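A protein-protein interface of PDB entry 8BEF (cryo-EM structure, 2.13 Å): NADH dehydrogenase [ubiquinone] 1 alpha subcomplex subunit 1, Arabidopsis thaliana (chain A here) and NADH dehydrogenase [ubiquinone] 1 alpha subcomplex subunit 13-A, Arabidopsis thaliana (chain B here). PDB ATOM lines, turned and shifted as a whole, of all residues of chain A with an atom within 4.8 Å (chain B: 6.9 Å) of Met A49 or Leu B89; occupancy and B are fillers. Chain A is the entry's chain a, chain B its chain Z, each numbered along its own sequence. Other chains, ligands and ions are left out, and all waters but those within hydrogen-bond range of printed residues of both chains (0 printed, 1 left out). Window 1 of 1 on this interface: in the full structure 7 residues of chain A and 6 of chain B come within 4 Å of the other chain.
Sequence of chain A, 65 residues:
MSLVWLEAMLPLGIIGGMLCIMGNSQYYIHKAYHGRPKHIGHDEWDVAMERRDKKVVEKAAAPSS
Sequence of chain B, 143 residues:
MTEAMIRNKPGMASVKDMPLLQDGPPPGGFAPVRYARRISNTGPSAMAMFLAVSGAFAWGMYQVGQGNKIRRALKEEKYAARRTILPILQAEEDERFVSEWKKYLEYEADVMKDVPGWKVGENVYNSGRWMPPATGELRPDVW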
ATOM      1  N   TRP A  45     -23.643  10.374 -11.483  1.00  0.00           N
ATOM      2  CA  TRP A  45     -24.937   9.716 -11.612  1.00  0.00           C
ATOM      3  C   TRP A  45     -25.349   9.582 -13.073  1.00  0.00           C
ATOM      4  O   TRP A  45     -25.814   8.522 -13.501  1.00  0.00           O
ATOM      5  CB  TRP A  45     -25.995  10.490 -10.824  1.00  0.00           C
ATOM      6  CG  TRP A  45     -27.365   9.893 -10.908  1.00  0.00           C
ATOM      7  CD1 TRP A  45     -28.297  10.115 -11.874  1.00  0.00           C
ATOM      8  CD2 TRP A  45     -27.955   8.971  -9.984  1.00  0.00           C
ATOM      9  NE1 TRP A  45     -29.434   9.390 -11.612  1.00  0.00           N
ATOM     10  CE2 TRP A  45     -29.250   8.680 -10.457  1.00  0.00           C
ATOM     11  CE3 TRP A  45     -27.516   8.365  -8.803  1.00  0.00           C
ATOM     12  CZ2 TRP A  45     -30.109   7.809  -9.790  1.00  0.00           C
ATOM     13  CZ3 TRP A  45     -28.370   7.502  -8.144  1.00  0.00           C
ATOM     14  CH2 TRP A  45     -29.651   7.230  -8.640  1.00  0.00           C
ATOM     15  N   ASP A  46     -25.190  10.652 -13.854  1.00  0.00           N
ATOM     16  CA  ASP A  46     -25.594  10.607 -15.257  1.00  0.00           C
ATOM     17  C   ASP A  46     -24.744   9.621 -16.050  1.00  0.00           C
ATOM     18  O   ASP A  46     -25.260   8.893 -16.905  1.00  0.00           O
ATOM     19  CB  ASP A  46     -25.517  12.006 -15.868  1.00  0.00           C
ATOM     20  CG  ASP A  46     -26.474  12.983 -15.210  1.00  0.00           C
ATOM     21  OD1 ASP A  46     -27.643  12.615 -14.982  1.00  0.00           O
ATOM     22  OD2 ASP A  46     -26.057  14.119 -14.915  1.00  0.00           O
ATOM     23  N   VAL A  47     -23.438   9.582 -15.775  1.00  0.00           N
ATOM     24  CA  VAL A  47     -22.551   8.642 -16.456  1.00  0.00           C
ATOM     25  C   VAL A  47     -22.932   7.203 -16.122  1.00  0.00           C
ATOM     26  O   VAL A  47     -22.986   6.336 -17.006  1.00  0.00           O
ATOM     27  CB  VAL A  47     -21.084   8.948 -16.097  1.00  0.00           C
ATOM     28  CG1 VAL A  47     -20.163   7.906 -16.681  1.00  0.00           C
ATOM     29  CG2 VAL A  47     -20.694  10.330 -16.599  1.00  0.00           C
ATOM     30  N   ALA A  48     -23.195   6.924 -14.841  1.00  0.00           N
ATOM     31  CA  ALA A  48     -23.634   5.586 -14.453  1.00  0.00           C
ATOM     32  C   ALA A  48     -24.969   5.232 -15.100  1.00  0.00           C
ATOM     33  O   ALA A  48     -25.182   4.087 -15.515  1.00  0.00           O
ATOM     34  CB  ALA A  48     -23.729   5.482 -12.930  1.00  0.00           C
ATOM     35  N   MET A  49     -25.878   6.206 -15.199  1.00  0.00           N
ATOM     36  CA  MET A  49     -27.156   5.980 -15.865  1.00  0.00           C
ATOM     37  C   MET A  49     -26.965   5.606 -17.327  1.00  0.00           C
ATOM     38  O   MET A  49     -27.592   4.667 -17.820  1.00  0.00           O
ATOM     39  CB  MET A  49     -28.044   7.220 -15.742  1.00  0.00           C
ATOM     40  CG  MET A  49     -28.737   7.491 -14.389  1.00  0.00           C
ATOM     41  SD  MET A  49     -29.420   6.121 -13.413  1.00  0.00           S
ATOM     42  CE  MET A  49     -27.977   5.336 -12.702  1.00  0.00           C
ATOM     43  N   GLU A  50     -26.106   6.336 -18.041  1.00  0.00           N
ATOM     44  CA  GLU A  50     -25.868   6.024 -19.448  1.00  0.00           C
ATOM     45  C   GLU A  50     -25.219   4.653 -19.622  1.00  0.00           C
ATOM     46  O   GLU A  50     -25.615   3.877 -20.505  1.00  0.00           O
ATOM     47  CB  GLU A  50     -25.019   7.122 -20.091  1.00  0.00           C
ATOM     48  CG  GLU A  50     -25.730   8.465 -20.197  1.00  0.00           C
ATOM     49  CD  GLU A  50     -24.861   9.571 -20.768  1.00  0.00           C
ATOM     50  OE1 GLU A  50     -23.638   9.345 -20.911  1.00  0.00           O
ATOM     51  OE2 GLU A  50     -25.384  10.670 -21.043  1.00  0.00           O
ATOM     52  N   ARG A  51     -24.234   4.326 -18.780  1.00  0.00           N
ATOM     53  CA  ARG A  51     -23.587   3.022 -18.896  1.00  0.00           C
ATOM     54  C   ARG A  51     -24.567   1.887 -18.613  1.00  0.00           C
ATOM     55  O   ARG A  51     -24.564   0.872 -19.318  1.00  0.00           O
ATOM     56  CB  ARG A  51     -22.378   2.934 -17.964  1.00  0.00           C
ATOM     57  CG  ARG A  51     -21.125   3.590 -18.522  1.00  0.00           C
ATOM     58  CD  ARG A  51     -20.265   4.169 -17.416  1.00  0.00           C
ATOM     59  NE  ARG A  51     -19.251   5.084 -17.925  1.00  0.00           N
ATOM     60  CZ  ARG A  51     -18.061   5.266 -17.370  1.00  0.00           C
ATOM     61  NH1 ARG A  51     -17.687   4.587 -16.298  1.00  0.00           N
ATOM     62  NH2 ARG A  51     -17.230   6.157 -17.899  1.00  0.00           N
ATOM     63  N   ARG A  52     -25.414   2.034 -17.592  1.00  0.00           N
ATOM     64  CA  ARG A  52     -26.398   0.995 -17.305  1.00  0.00           C
ATOM     65  C   ARG A  52     -27.490   0.944 -18.371  1.00  0.00           C
ATOM     66  O   ARG A  52     -28.007  -0.138 -18.682  1.00  0.00           O
ATOM     67  CB  ARG A  52     -26.989   1.223 -15.914  1.00  0.00           C
ATOM     68  CG  ARG A  52     -28.149   0.328 -15.553  1.00  0.00           C
ATOM     69  CD  ARG A  52     -29.244   1.124 -14.878  1.00  0.00           C
ATOM     70  NE  ARG A  52     -30.480   0.367 -14.736  1.00  0.00           N
ATOM     71  CZ  ARG A  52     -31.616   0.674 -15.346  1.00  0.00           C
ATOM     72  NH1 ARG A  52     -31.702   1.708 -16.166  1.00  0.00           N
ATOM     73  NH2 ARG A  52     -32.692  -0.077 -15.131  1.00  0.00           N
ATOM     74  N   ASP A  53     -27.827   2.092 -18.963  1.00  0.00           N
ATOM     75  CA  ASP A  53     -28.862   2.134 -19.988  1.00  0.00           C
ATOM     76  C   ASP A  53     -28.402   1.465 -21.269  1.00  0.00           C
ATOM     77  O   ASP A  53     -29.228   0.904 -21.995  1.00  0.00           O
ATOM     78  CB  ASP A  53     -29.275   3.579 -20.266  1.00  0.00           C
ATOM     79  CG  ASP A  53     -30.522   3.981 -19.510  1.00  0.00           C
ATOM     80  OD1 ASP A  53     -30.824   3.336 -18.485  1.00  0.00           O
ATOM     81  OD2 ASP A  53     -31.197   4.941 -19.933  1.00  0.00           O
ATOM     82  N   ARG B  82     -33.642  11.336  -7.779  1.00  0.00           N
ATOM     83  CA  ARG B  82     -32.615  10.301  -7.719  1.00  0.00           C
ATOM     84  C   ARG B  82     -32.802   9.387  -6.514  1.00  0.00           C
ATOM     85  O   ARG B  82     -32.441   8.206  -6.568  1.00  0.00           O
ATOM     86  CB  ARG B  82     -31.228  10.934  -7.697  1.00  0.00           C
ATOM     87  CG  ARG B  82     -30.795  11.462  -9.044  1.00  0.00           C
ATOM     88  CD  ARG B  82     -29.584  12.354  -8.925  1.00  0.00           C
ATOM     89  NE  ARG B  82     -29.171  12.868 -10.222  1.00  0.00           N
ATOM     90  CZ  ARG B  82     -27.964  13.348 -10.484  1.00  0.00           C
ATOM     91  NH1 ARG B  82     -27.031  13.420  -9.548  1.00  0.00           N
ATOM     92  NH2 ARG B  82     -27.684  13.760 -11.717  1.00  0.00           N
ATOM     93  N   ILE B  85     -35.653   6.412  -7.066  1.00  0.00           N
ATOM     94  CA  ILE B  85     -35.298   5.320  -7.967  1.00  0.00           C
ATOM     95  C   ILE B  85     -33.985   4.656  -7.588  1.00  0.00           C
ATOM     96  O   ILE B  85     -33.550   3.722  -8.275  1.00  0.00           O
ATOM     97  CB  ILE B  85     -35.251   5.792  -9.434  1.00  0.00           C
ATOM     98  CG1 ILE B  85     -34.097   6.776  -9.655  1.00  0.00           C
ATOM     99  CG2 ILE B  85     -36.580   6.399  -9.840  1.00  0.00           C
ATOM    100  CD1 ILE B  85     -33.701   6.930 -11.100  1.00  0.00           C
ATOM    101  N   LEU B  86     -33.340   5.110  -6.515  1.00  0.00           N
ATOM    102  CA  LEU B  86     -32.115   4.468  -6.045  1.00  0.00           C
ATOM    103  C   LEU B  86     -32.298   2.983  -5.739  1.00  0.00           C
ATOM    104  O   LEU B  86     -31.465   2.178  -6.194  1.00  0.00           O
ATOM    105  CB  LEU B  86     -31.591   5.237  -4.825  1.00  0.00           C
ATOM    106  CG  LEU B  86     -30.290   4.843  -4.123  1.00  0.00           C
ATOM    107  CD1 LEU B  86     -30.500   3.765  -3.078  1.00  0.00           C
ATOM    108  CD2 LEU B  86     -29.287   4.394  -5.124  1.00  0.00           C
ATOM    109  N   PRO B  87     -33.316   2.553  -4.980  1.00  0.00           N
ATOM    110  CA  PRO B  87     -33.384   1.126  -4.610  1.00  0.00           C
ATOM    111  C   PRO B  87     -33.456   0.166  -5.785  1.00  0.00           C
ATOM    112  O   PRO B  87     -32.800  -0.879  -5.740  1.00  0.00           O
ATOM    113  CB  PRO B  87     -34.646   1.059  -3.738  1.00  0.00           C
ATOM    114  CG  PRO B  87     -34.777   2.419  -3.182  1.00  0.00           C
ATOM    115  CD  PRO B  87     -34.354   3.333  -4.280  1.00  0.00           C
ATOM    116  N   ILE B  88     -34.211   0.480  -6.840  1.00  0.00           N
ATOM    117  CA  ILE B  88     -34.328  -0.465  -7.948  1.00  0.00           C
ATOM    118  C   ILE B  88     -33.017  -0.559  -8.724  1.00  0.00           C
ATOM    119  O   ILE B  88     -32.599  -1.650  -9.136  1.00  0.00           O
ATOM    120  CB  ILE B  88     -35.517  -0.103  -8.861  1.00  0.00           C
ATOM    121  CG1 ILE B  88     -35.728  -1.210  -9.896  1.00  0.00           C
ATOM    122  CG2 ILE B  88     -35.332   1.258  -9.525  1.00  0.00           C
ATOM    123  CD1 ILE B  88     -36.786  -0.913 -10.914  1.00  0.00           C
ATOM    124  N   LEU B  89     -32.335   0.573  -8.917  1.00  0.00           N
ATOM    125  CA  LEU B  89     -31.027   0.540  -9.564  1.00  0.00           C
ATOM    126  C   LEU B  89     -30.034  -0.272  -8.744  1.00  0.00           C
ATOM    127  O   LEU B  89     -29.276  -1.084  -9.294  1.00  0.00           O
ATOM    128  CB  LEU B  89     -30.519   1.966  -9.781  1.00  0.00           C
ATOM    129  CG  LEU B  89     -31.421   2.860 -10.636  1.00  0.00           C
ATOM    130  CD1 LEU B  89     -31.039   4.328 -10.500  1.00  0.00           C
ATOM    131  CD2 LEU B  89     -31.383   2.424 -12.097  1.00  0.00           C
ATOM    132  N   GLN B  90     -30.039  -0.083  -7.422  1.00  0.00           N
ATOM    133  CA  GLN B  90     -29.135  -0.843  -6.567  1.00  0.00           C
ATOM    134  C   GLN B  90     -29.460  -2.333  -6.599  1.00  0.00           C
ATOM    135  O   GLN B  90     -28.552  -3.163  -6.595  1.00  0.00           O
ATOM    136  CB  GLN B  90     -29.189  -0.317  -5.134  1.00  0.00           C
ATOM    137  CG  GLN B  90     -27.931  -0.588  -4.326  1.00  0.00           C
ATOM    138  CD  GLN B  90     -26.659  -0.411  -5.132  1.00  0.00           C
ATOM    139  OE1 GLN B  90     -26.294   0.704  -5.496  1.00  0.00           O
ATOM    140  NE2 GLN B  90     -25.972  -1.511  -5.409  1.00  0.00           N
ATOM    141  N   ALA B  91     -30.747  -2.687  -6.614  1.00  0.00           N
ATOM    142  CA  ALA B  91     -31.133  -4.096  -6.658  1.00  0.00           C
ATOM    143  C   ALA B  91     -30.689  -4.749  -7.961  1.00  0.00           C
ATOM    144  O   ALA B  91     -30.182  -5.880  -7.961  1.00  0.00           O
ATOM    145  CB  ALA B  91     -32.644  -4.226  -6.479  1.00  0.00           C
ATOM    146  N   GLU B  92     -30.875  -4.049  -9.082  1.00  0.00           N
ATOM    147  CA  GLU B  92     -30.370  -4.536 -10.361  1.00  0.00           C
ATOM    148  C   GLU B  92     -28.862  -4.749 -10.308  1.00  0.00           C
ATOM    149  O   GLU B  92     -28.351  -5.790 -10.746  1.00  0.00           O
ATOM    150  CB  GLU B  92     -30.731  -3.542 -11.461  1.00  0.00           C
ATOM    151  CG  GLU B  92     -30.312  -3.956 -12.848  1.00  0.00           C
ATOM    152  CD  GLU B  92     -30.662  -2.905 -13.879  1.00  0.00           C
ATOM    153  OE1 GLU B  92     -31.821  -2.883 -14.336  1.00  0.00           O
ATOM    154  OE2 GLU B  92     -29.776  -2.102 -14.235  1.00  0.00           O
ATOM    155  N   GLU B  93     -28.131  -3.769  -9.768  1.00  0.00           N
ATOM    156  CA  GLU B  93     -26.682  -3.899  -9.681  1.00  0.00           C
ATOM    157  C   GLU B  93     -26.284  -5.066  -8.784  1.00  0.00           C
ATOM    158  O   GLU B  93     -25.312  -5.773  -9.070  1.00  0.00           O
ATOM    159  CB  GLU B  93     -26.060  -2.593  -9.178  1.00  0.00           C
ATOM    160  CG  GLU B  93     -24.588  -2.707  -8.797  1.00  0.00           C
ATOM    161  CD  GLU B  93     -23.659  -2.934  -9.984  1.00  0.00           C
ATOM    162  OE1 GLU B  93     -24.138  -3.034 -11.133  1.00  0.00           O
ATOM    163  OE2 GLU B  93     -22.437  -3.032  -9.760  1.00  0.00           O
ATOM    164  N   ASP B  94     -27.023  -5.279  -7.695  1.00  0.00           N
ATOM    165  CA  ASP B  94     -26.717  -6.382  -6.791  1.00  0.00           C
ATOM    166  C   ASP B  94     -26.902  -7.724  -7.486  1.00  0.00           C
ATOM    167  O   ASP B  94     -26.054  -8.616  -7.373  1.00  0.00           O
ATOM    168  CB  ASP B  94     -27.597  -6.297  -5.543  1.00  0.00           C
ATOM    169  CG  ASP B  94     -27.107  -5.260  -4.552  1.00  0.00           C
ATOM    170  OD1 ASP B  94     -26.039  -4.660  -4.792  1.00  0.00           O
ATOM    171  OD2 ASP B  94     -27.787  -5.057  -3.525  1.00  0.00           O
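Of the 11 printed residues of chain B, 4 touch a printed residue of chain A.
Along chain B the printed residues that touch a printed residue of chain A span positions 82 to 92.
Of the 9 printed residues of chain A, 4 touch a printed residue of chain B.
Hydrophobic or aromatic side chains of chain A within 4 Å of the printed part of chain B: Trp A45 and Met A49.
OD1 of Asp A53 is in salt-bridge range of NH1 of Arg A52.
The indole nitrogen of Trp A45 sits close to the side-chain sulfur of Met A49 (3.7 Å).
Met A49 touches one residue of chain B.
Leu B89 touches just these residues of chain A: Trp A45 (3.7 Å), Met A49 (3.8 Å) and Arg A52 (3.5 Å).
Of the printed residues of chain B, Arg A52 touches Leu B89 (3.5 Å) and Glu B92 (2.6 Å).
Printed residues of chain A within 4 Å of Ile B85: Trp A45 (3.9 Å).
Of the printed residues of chain B, Asp A46 touches Arg B82.
Ala B91 touches none of the printed residues of chain A.
Glu B93 touches none of the printed residues of chain A.
The nearest residue of chain B that does not touch Met A49 is Ile B85 (4.9 Å).
The nearest printed residue of chain A that does not touch Leu B89 is Asp A53 (6.5 Å).
The nearest printed residue of chain B that does not touch Trp A45 is Leu B86 (4.4 Å).
The guanidinium group of Arg A52 lies within salt-bridge range of the side-chain carboxylate of Glu B92.
NH2 of Arg B82 lies within salt-bridge range of OD1 of Asp A46 (3.5 Å).
Among the printed residues, merely in contact across the chains: Trp A45 with Arg B82 (3.3 Å), Arg A52 with Leu B89 (3.5 Å), Trp A45 with Leu B89 (3.7 Å), Met A49 with Leu B89 (3.8 Å) and Trp A45 with Ile B85 (3.9 Å).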
